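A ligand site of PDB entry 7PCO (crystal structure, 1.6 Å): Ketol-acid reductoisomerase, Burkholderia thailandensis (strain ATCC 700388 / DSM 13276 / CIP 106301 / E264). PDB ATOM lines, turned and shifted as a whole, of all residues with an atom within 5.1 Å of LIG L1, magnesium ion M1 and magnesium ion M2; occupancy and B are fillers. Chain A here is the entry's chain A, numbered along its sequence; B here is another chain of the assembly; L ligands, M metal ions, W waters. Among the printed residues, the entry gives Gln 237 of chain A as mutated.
The side-chain hydroxyl (OG) of Ser 259 sits close to an oxygen (O1) of LIG L1 (3.5 Å).
O of Gln 257 is in hydrogen-bond range of N7 of LG2 L2, 3.1 Å away.
NE2 of Gln 237 sits close to O4 of LIG L1, 2.7 Å away.
The backbone NH (N) of Ser 259 lies within hydrogen-bond range of an oxygen (O1) of LIG L1.
An oxygen (O1) of LIG L1 is in hydrogen-bond range of a nitrogen (N7) of LG2 L2.
The side-chain hydroxyl (OH) of Tyr 138 of chain B is in hydrogen-bond range of the backbone NH (N) of Met 241 (3.4 Å).
OE1 of Gln 237 lies close to OE1 of Gln 199 of chain B (2.8 Å).
NE2 of Gln 199 of chain B is in hydrogen-bond range of O of Glu 231 (2.8 Å).
The guanidinium group of Arg 136 of chain B is in salt-bridge range of the side-chain carboxylate of Glu 231 (2.8 Å).
OG of Ser 259 sits at hydrogen-bond distance from N of Cys 262 (3.1 Å).
The guanidinium group of Arg 136 of chain B lies close to the side-chain carboxylate of Asp 196 of chain B (2.9 Å).
O of Gln 257 touches C8 of LIG L1, at 3.9 Å.
Gly 258 touches LIG L1 (CA to O1, 3.6 Å).
Cys 262 touches LIG L1 (CB to O1, 3.3 Å).
Tyr 138 of chain B touches LIG L1.
Hydrophobic or aromatic side chains that line LIG L1: Tyr 138 of chain B.
Eight residues have an atom within 4 Å of LIG L1: Gln 237, Gln 257, Gly 258, Ser 259, Cys 262, Tyr 138 of chain B, Asp 196 of chain B and Glu 200 of chain B.
Residues that only touch magnesium ion M1: Gln 199 of chain B, Arg 136 of chain B and Gln 237.
The nearest printed residue that does not touch magnesium ion M2 is Ser 259 (4.3 Å).
Magnesium ion M1 is bound by water W5 (2.0 Å), the side-chain carboxylate (OD1) of Asp 196 of chain B (2.0 Å), an oxygen (O3) of LIG L1 (2.0 Å), water W3 (2.1 Å), water W1 (2.2 Å) and an oxygen (O4) of LIG L1 (2.3 Å).
Magnesium ion M2 is bound by OD2 of Asp 196 of chain B, OE2 of Glu 200 of chain B, water W4, O3 of LIG L1, water W2 and O2 of LIG L1.
Magnesium ion M2 has six donor atoms within binding distance.
Water W5 bridges the backbone carbonyl oxygen of Pro 135 of chain B (2.7 Å) and the guanidinium group of Arg 136 of chain B (3.3 Å).
Water W2 lies within hydrogen-bond range of the side-chain carboxylate of Glu 200 of chain B (2.8 Å) and a ring nitrogen (NE2) of His 113 of chain B (3.2 Å).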
ATOM      1  N   GLU A 231     -19.741 -26.737 -31.604  1.00  0.00           N
ATOM      2  CA  GLU A 231     -19.270 -27.074 -30.230  1.00  0.00           C
ATOM      3  C   GLU A 231     -17.828 -27.572 -30.253  1.00  0.00           C
ATOM      4  O   GLU A 231     -17.086 -27.185 -29.359  1.00  0.00           O
ATOM      5  CB  GLU A 231     -20.212 -28.078 -29.573  1.00  0.00           C
ATOM      6  CG  GLU A 231     -21.608 -27.519 -29.463  1.00  0.00           C
ATOM      7  CD  GLU A 231     -21.625 -26.093 -28.946  1.00  0.00           C
ATOM      8  OE1 GLU A 231     -21.064 -25.877 -27.844  1.00  0.00           O
ATOM      9  OE2 GLU A 231     -22.149 -25.221 -29.633  1.00  0.00           O
ATOM     10  N   GLN A 237     -15.182 -21.313 -29.102  1.00  0.00           N
ATOM     11  CA  GLN A 237     -15.073 -21.510 -27.641  1.00  0.00           C
ATOM     12  C   GLN A 237     -13.830 -22.337 -27.314  1.00  0.00           C
ATOM     13  O   GLN A 237     -13.109 -21.958 -26.384  1.00  0.00           O
ATOM     14  CB  GLN A 237     -16.309 -22.172 -27.024  1.00  0.00           C
ATOM     15  CG  GLN A 237     -16.247 -22.125 -25.509  1.00  0.00           C
ATOM     16  CD  GLN A 237     -17.541 -22.494 -24.849  1.00  0.00           C
ATOM     17  OE1 GLN A 237     -17.998 -23.632 -24.918  1.00  0.00           O
ATOM     18  NE2 GLN A 237     -18.127 -21.534 -24.159  1.00  0.00           N
ATOM     19  N   MET A 238     -13.596 -23.458 -28.010  1.00  0.00           N
ATOM     20  CA  MET A 238     -12.443 -24.337 -27.656  1.00  0.00           C
ATOM     21  C   MET A 238     -11.118 -23.587 -27.919  1.00  0.00           C
ATOM     22  O   MET A 238     -10.217 -23.656 -27.045  1.00  0.00           O
ATOM     23  CB  MET A 238     -12.525 -25.660 -28.403  1.00  0.00           C
ATOM     24  CG  MET A 238     -13.694 -26.524 -27.937  1.00  0.00           C
ATOM     25  SD  MET A 238     -13.522 -27.075 -26.216  1.00  0.00           S
ATOM     26  CE  MET A 238     -14.449 -25.814 -25.341  1.00  0.00           C
ATOM     27  N   MET A 241     -10.704 -20.875 -25.144  1.00  0.00           N
ATOM     28  CA  MET A 241     -10.257 -21.568 -23.906  1.00  0.00           C
ATOM     29  C   MET A 241      -8.743 -21.817 -23.996  1.00  0.00           C
ATOM     30  O   MET A 241      -8.017 -21.533 -23.014  1.00  0.00           O
ATOM     31  CB  MET A 241     -10.999 -22.899 -23.730  1.00  0.00           C
ATOM     32  CG  MET A 241     -10.553 -23.705 -22.516  1.00  0.00           C
ATOM     33  SD  MET A 241     -11.279 -25.363 -22.507  1.00  0.00           S
ATOM     34  CE  MET A 241     -10.216 -26.145 -23.718  1.00  0.00           C
ATOM     35  N   VAL A 253      -8.874 -21.463 -16.621  1.00  0.00           N
ATOM     36  CA  VAL A 253      -9.961 -20.943 -17.516  1.00  0.00           C
ATOM     37  C   VAL A 253     -11.275 -21.631 -17.131  1.00  0.00           C
ATOM     38  O   VAL A 253     -12.296 -20.942 -17.033  1.00  0.00           O
ATOM     39  CB  VAL A 253      -9.632 -21.137 -19.003  1.00  0.00           C
ATOM     40  CG1 VAL A 253     -10.846 -20.895 -19.886  1.00  0.00           C
ATOM     41  CG2 VAL A 253      -8.485 -20.250 -19.422  1.00  0.00           C
ATOM     42  N   VAL A 254     -11.253 -22.944 -16.885  1.00  0.00           N
ATOM     43  CA  VAL A 254     -12.508 -23.683 -16.538  1.00  0.00           C
ATOM     44  C   VAL A 254     -13.015 -23.208 -15.169  1.00  0.00           C
ATOM     45  O   VAL A 254     -14.216 -22.978 -15.035  1.00  0.00           O
ATOM     46  CB  VAL A 254     -12.285 -25.208 -16.619  1.00  0.00           C
ATOM     47  CG1 VAL A 254     -13.458 -25.991 -16.048  1.00  0.00           C
ATOM     48  CG2 VAL A 254     -12.016 -25.612 -18.058  1.00  0.00           C
ATOM     49  N   GLN A 257     -14.354 -19.412 -15.858  1.00  0.00           N
ATOM     50  CA  GLN A 257     -15.340 -19.094 -16.926  1.00  0.00           C
ATOM     51  C   GLN A 257     -16.415 -20.178 -17.022  1.00  0.00           C
ATOM     52  O   GLN A 257     -17.410 -19.916 -17.728  1.00  0.00           O
ATOM     53  CB  GLN A 257     -14.665 -18.987 -18.293  1.00  0.00           C
ATOM     54  CG  GLN A 257     -13.530 -17.984 -18.331  1.00  0.00           C
ATOM     55  CD  GLN A 257     -14.009 -16.559 -18.204  1.00  0.00           C
ATOM     56  OE1 GLN A 257     -15.091 -16.275 -17.671  1.00  0.00           O
ATOM     57  NE2 GLN A 257     -13.203 -15.648 -18.710  1.00  0.00           N
ATOM     58  N   GLY A 258     -16.194 -21.346 -16.427  1.00  0.00           N
ATOM     59  CA  GLY A 258     -17.154 -22.461 -16.491  1.00  0.00           C
ATOM     60  C   GLY A 258     -18.284 -22.304 -15.477  1.00  0.00           C
ATOM     61  O   GLY A 258     -17.990 -21.995 -14.305  1.00  0.00           O
ATOM     62  N   SER A 259     -19.532 -22.571 -15.877  1.00  0.00           N
ATOM     63  CA  SER A 259     -20.664 -22.773 -14.935  1.00  0.00           C
ATOM     64  C   SER A 259     -20.273 -23.899 -13.989  1.00  0.00           C
ATOM     65  O   SER A 259     -19.416 -24.718 -14.302  1.00  0.00           O
ATOM     66  CB  SER A 259     -21.966 -23.112 -15.641  1.00  0.00           C
ATOM     67  OG  SER A 259     -21.905 -24.437 -16.176  1.00  0.00           O
ATOM     68  N   CYS A 262     -20.504 -27.164 -15.809  1.00  0.00           N
ATOM     69  CA  CYS A 262     -19.324 -27.335 -16.688  1.00  0.00           C
ATOM     70  C   CYS A 262     -18.144 -27.856 -15.856  1.00  0.00           C
ATOM     71  O   CYS A 262     -17.546 -28.885 -16.234  1.00  0.00           O
ATOM     72  CB  CYS A 262     -18.972 -26.024 -17.381  1.00  0.00           C
ATOM     73  SG  CYS A 262     -17.399 -26.124 -18.266  1.00  0.00           S
ATOM     74  N   HIS B 113     -29.418 -22.889 -20.799  1.00  0.00           N
ATOM     75  CA  HIS B 113     -28.994 -24.323 -20.883  1.00  0.00           C
ATOM     76  C   HIS B 113     -30.258 -25.164 -20.654  1.00  0.00           C
ATOM     77  O   HIS B 113     -31.097 -24.757 -19.812  1.00  0.00           O
ATOM     78  CB  HIS B 113     -27.898 -24.598 -19.848  1.00  0.00           C
ATOM     79  CG  HIS B 113     -27.314 -25.983 -19.829  1.00  0.00           C
ATOM     80  ND1 HIS B 113     -27.130 -26.754 -20.956  1.00  0.00           N
ATOM     81  CD2 HIS B 113     -26.755 -26.670 -18.805  1.00  0.00           C
ATOM     82  CE1 HIS B 113     -26.536 -27.897 -20.613  1.00  0.00           C
ATOM     83  NE2 HIS B 113     -26.311 -27.869 -19.287  1.00  0.00           N
ATOM     84  N   PRO B 135     -26.129 -19.391 -25.224  1.00  0.00           N
ATOM     85  CA  PRO B 135     -24.926 -18.896 -25.882  1.00  0.00           C
ATOM     86  C   PRO B 135     -23.883 -20.012 -26.038  1.00  0.00           C
ATOM     87  O   PRO B 135     -23.853 -20.897 -25.208  1.00  0.00           O
ATOM     88  CB  PRO B 135     -24.415 -17.775 -24.966  1.00  0.00           C
ATOM     89  CG  PRO B 135     -25.628 -17.399 -24.128  1.00  0.00           C
ATOM     90  CD  PRO B 135     -26.364 -18.708 -23.932  1.00  0.00           C
ATOM     91  N   ARG B 136     -23.064 -19.927 -27.090  1.00  0.00           N
ATOM     92  CA  ARG B 136     -22.034 -20.946 -27.391  1.00  0.00           C
ATOM     93  C   ARG B 136     -20.659 -20.411 -26.987  1.00  0.00           C
ATOM     94  O   ARG B 136     -19.663 -20.937 -27.469  1.00  0.00           O
ATOM     95  CB  ARG B 136     -22.049 -21.329 -28.860  1.00  0.00           C
ATOM     96  CG  ARG B 136     -23.410 -21.745 -29.396  1.00  0.00           C
ATOM     97  CD  ARG B 136     -24.287 -22.472 -28.403  1.00  0.00           C
ATOM     98  NE  ARG B 136     -23.730 -23.696 -27.839  1.00  0.00           N
ATOM     99  CZ  ARG B 136     -24.277 -24.363 -26.817  1.00  0.00           C
ATOM    100  NH1 ARG B 136     -25.395 -23.928 -26.269  1.00  0.00           N
ATOM    101  NH2 ARG B 136     -23.719 -25.488 -26.382  1.00  0.00           N
ATOM    102  N   MET B 137     -20.627 -19.456 -26.062  1.00  0.00           N
ATOM    103  CA  MET B 137     -19.380 -18.766 -25.652  1.00  0.00           C
ATOM    104  C   MET B 137     -19.564 -18.248 -24.231  1.00  0.00           C
ATOM    105  O   MET B 137     -20.710 -17.970 -23.831  1.00  0.00           O
ATOM    106  CB  MET B 137     -19.129 -17.585 -26.596  1.00  0.00           C
ATOM    107  CG  MET B 137     -17.852 -16.817 -26.328  1.00  0.00           C
ATOM    108  SD  MET B 137     -16.369 -17.811 -26.517  1.00  0.00           S
ATOM    109  CE  MET B 137     -16.556 -18.316 -28.223  1.00  0.00           C
ATOM    110  N   TYR B 138     -18.465 -18.080 -23.508  1.00  0.00           N
ATOM    111  CA  TYR B 138     -18.473 -17.536 -22.125  1.00  0.00           C
ATOM    112  C   TYR B 138     -18.534 -15.998 -22.208  1.00  0.00           C
ATOM    113  O   TYR B 138     -18.534 -15.429 -23.306  1.00  0.00           O
ATOM    114  CB  TYR B 138     -17.352 -18.149 -21.278  1.00  0.00           C
ATOM    115  CG  TYR B 138     -15.950 -18.196 -21.827  1.00  0.00           C
ATOM    116  CD1 TYR B 138     -15.040 -17.186 -21.554  1.00  0.00           C
ATOM    117  CD2 TYR B 138     -15.483 -19.321 -22.487  1.00  0.00           C
ATOM    118  CE1 TYR B 138     -13.721 -17.257 -21.988  1.00  0.00           C
ATOM    119  CE2 TYR B 138     -14.178 -19.403 -22.934  1.00  0.00           C
ATOM    120  CZ  TYR B 138     -13.289 -18.376 -22.684  1.00  0.00           C
ATOM    121  OH  TYR B 138     -11.996 -18.498 -23.112  1.00  0.00           O
ATOM    122  N   ASP B 196     -23.988 -29.755 -25.187  1.00  0.00           N
ATOM    123  CA  ASP B 196     -23.218 -28.844 -24.301  1.00  0.00           C
ATOM    124  C   ASP B 196     -22.440 -29.659 -23.264  1.00  0.00           C
ATOM    125  O   ASP B 196     -21.249 -29.407 -23.089  1.00  0.00           O
ATOM    126  CB  ASP B 196     -24.167 -27.855 -23.621  1.00  0.00           C
ATOM    127  CG  ASP B 196     -23.432 -26.706 -22.963  1.00  0.00           C
ATOM    128  OD1 ASP B 196     -22.731 -25.973 -23.694  1.00  0.00           O
ATOM    129  OD2 ASP B 196     -23.568 -26.566 -21.734  1.00  0.00           O
ATOM    130  N   GLN B 199     -19.376 -31.483 -24.823  1.00  0.00           N
ATOM    131  CA  GLN B 199     -18.260 -30.514 -24.993  1.00  0.00           C
ATOM    132  C   GLN B 199     -17.480 -30.407 -23.682  1.00  0.00           C
ATOM    133  O   GLN B 199     -16.224 -30.344 -23.731  1.00  0.00           O
ATOM    134  CB  GLN B 199     -18.810 -29.144 -25.401  1.00  0.00           C
ATOM    135  CG  GLN B 199     -17.732 -28.150 -25.822  1.00  0.00           C
ATOM    136  CD  GLN B 199     -18.255 -26.726 -25.894  1.00  0.00           C
ATOM    137  OE1 GLN B 199     -18.997 -26.281 -25.028  1.00  0.00           O
ATOM    138  NE2 GLN B 199     -17.873 -26.011 -26.943  1.00  0.00           N
ATOM    139  N   GLU B 200     -18.182 -30.427 -22.544  1.00  0.00           N
ATOM    140  CA  GLU B 200     -17.582 -30.136 -21.208  1.00  0.00           C
ATOM    141  C   GLU B 200     -16.917 -31.394 -20.633  1.00  0.00           C
ATOM    142  O   GLU B 200     -15.938 -31.228 -19.875  1.00  0.00           O
ATOM    143  CB  GLU B 200     -18.650 -29.543 -20.291  1.00  0.00           C
ATOM    144  CG  GLU B 200     -19.191 -28.211 -20.788  1.00  0.00           C
ATOM    145  CD  GLU B 200     -20.489 -27.719 -20.167  1.00  0.00           C
ATOM    146  OE1 GLU B 200     -21.061 -28.457 -19.351  1.00  0.00           O
ATOM    147  OE2 GLU B 200     -20.933 -26.599 -20.515  1.00  0.00           O
HETATM  148  C1  LIG L   1     -21.022 -23.240 -20.786  1.00  0.00           C
HETATM  149  C2  LIG L   1     -19.794 -22.958 -21.580  1.00  0.00           C
HETATM  150  C3  LIG L   1     -18.797 -24.124 -21.611  1.00  0.00           C
HETATM  151  C4  LIG L   1     -16.260 -23.216 -21.335  1.00  0.00           C
HETATM  152  O1  LIG L   1     -19.905 -23.139 -18.672  1.00  0.00           O
HETATM  153  C5  LIG L   1     -20.830 -23.640 -19.292  1.00  0.00           C
HETATM  154  O2  LIG L   1     -21.658 -24.405 -18.828  1.00  0.00           O
HETATM  155  O3  LIG L   1     -21.745 -24.218 -21.453  1.00  0.00           O
HETATM  156  O4  LIG L   1     -20.163 -22.670 -22.893  1.00  0.00           O
HETATM  157  C6  LIG L   1     -17.672 -23.385 -20.829  1.00  0.00           C
HETATM  158  C7  LIG L   1     -15.525 -24.483 -21.114  1.00  0.00           C
HETATM  159  C8  LIG L   1     -15.616 -22.185 -20.382  1.00  0.00           C
HETATM  160  P1  LG2 L   2     -21.988 -18.564 -12.460  1.00  0.00           P
HETATM  161  O1  LG2 L   2     -21.323 -19.673 -11.693  1.00  0.00           O
HETATM  162  O2  LG2 L   2     -21.159 -17.421 -12.966  1.00  0.00           O
HETATM  163  O3  LG2 L   2     -23.210 -18.016 -11.610  1.00  0.00           O
HETATM  164  C1  LG2 L   2     -22.991 -17.116 -10.524  1.00  0.00           C
HETATM  165  C2  LG2 L   2     -24.282 -16.390 -10.302  1.00  0.00           C
HETATM  166  O4  LG2 L   2     -25.285 -17.313  -9.809  1.00  0.00           O
HETATM  167  C3  LG2 L   2     -24.224 -15.263  -9.273  1.00  0.00           C
HETATM  168  O5  LG2 L   2     -25.027 -14.192  -9.723  1.00  0.00           O
HETATM  169  C4  LG2 L   2     -24.734 -15.933  -8.001  1.00  0.00           C
HETATM  170  O6  LG2 L   2     -25.247 -14.998  -7.082  1.00  0.00           O
HETATM  171  C5  LG2 L   2     -25.806 -16.851  -8.582  1.00  0.00           C
HETATM  172  N1  LG2 L   2     -26.109 -18.005  -7.747  1.00  0.00           N
HETATM  173  C6  LG2 L   2     -25.286 -19.061  -7.462  1.00  0.00           C
HETATM  174  N2  LG2 L   2     -25.851 -19.951  -6.674  1.00  0.00           N
HETATM  175  C7  LG2 L   2     -27.130 -19.447  -6.459  1.00  0.00           C
HETATM  176  C8  LG2 L   2     -28.219 -19.928  -5.717  1.00  0.00           C
HETATM  177  N3  LG2 L   2     -28.212 -21.069  -5.026  1.00  0.00           N
HETATM  178  N4  LG2 L   2     -29.363 -19.197  -5.745  1.00  0.00           N
HETATM  179  C9  LG2 L   2     -29.365 -18.034  -6.417  1.00  0.00           C
HETATM  180  N5  LG2 L   2     -28.399 -17.488  -7.143  1.00  0.00           N
HETATM  181  C10 LG2 L   2     -27.289 -18.251  -7.120  1.00  0.00           C
HETATM  182  O7  LG2 L   2     -22.850 -19.246 -13.631  1.00  0.00           O
HETATM  183  P2  LG2 L   2     -22.880 -19.087 -15.223  1.00  0.00           P
HETATM  184  O8  LG2 L   2     -21.726 -19.808 -15.836  1.00  0.00           O
HETATM  185  O9  LG2 L   2     -23.066 -17.639 -15.538  1.00  0.00           O
HETATM  186  O10 LG2 L   2     -24.204 -19.913 -15.535  1.00  0.00           O
HETATM  187  C11 LG2 L   2     -25.525 -19.324 -15.577  1.00  0.00           C
HETATM  188  C12 LG2 L   2     -26.367 -20.087 -16.556  1.00  0.00           C
HETATM  189  O11 LG2 L   2     -25.810 -19.901 -17.873  1.00  0.00           O
HETATM  190  C13 LG2 L   2     -26.447 -21.613 -16.375  1.00  0.00           C
HETATM  191  O12 LG2 L   2     -27.726 -22.100 -16.754  1.00  0.00           O
HETATM  192  C14 LG2 L   2     -25.349 -22.115 -17.307  1.00  0.00           C
HETATM  193  O13 LG2 L   2     -25.490 -23.474 -17.660  1.00  0.00           O
HETATM  194  C15 LG2 L   2     -25.568 -21.162 -18.470  1.00  0.00           C
HETATM  195  N6  LG2 L   2     -24.419 -21.019 -19.421  1.00  0.00           N
HETATM  196  C16 LG2 L   2     -23.160 -20.688 -18.984  1.00  0.00           C
HETATM  197  C17 LG2 L   2     -22.169 -20.370 -19.902  1.00  0.00           C
HETATM  198  C18 LG2 L   2     -20.766 -19.964 -19.493  1.00  0.00           C
HETATM  199  O14 LG2 L   2     -19.963 -19.704 -20.384  1.00  0.00           O
HETATM  200  N7  LG2 L   2     -20.458 -19.896 -18.214  1.00  0.00           N
HETATM  201  C19 LG2 L   2     -22.463 -20.426 -21.268  1.00  0.00           C
HETATM  202  C20 LG2 L   2     -23.729 -20.765 -21.683  1.00  0.00           C
HETATM  203  C21 LG2 L   2     -24.660 -21.139 -20.745  1.00  0.00           C
HETATM  204 MG    MG M   1     -21.664 -24.316 -23.475  1.00  0.00          MG
HETATM  205 MG    MG M   2     -22.649 -25.589 -20.236  1.00  0.00          MG
HETATM  206  O   HOH W   1     -20.325 -26.019 -23.000  1.00  0.00           O
HETATM  207  O   HOH W   2     -23.308 -26.908 -18.817  1.00  0.00           O
HETATM  208  O   HOH W   3     -20.769 -24.275 -25.354  1.00  0.00           O
HETATM  209  O   HOH W   4     -24.350 -24.492 -20.014  1.00  0.00           O
HETATM  210  O   HOH W   5     -23.242 -23.193 -23.895  1.00  0.00           O
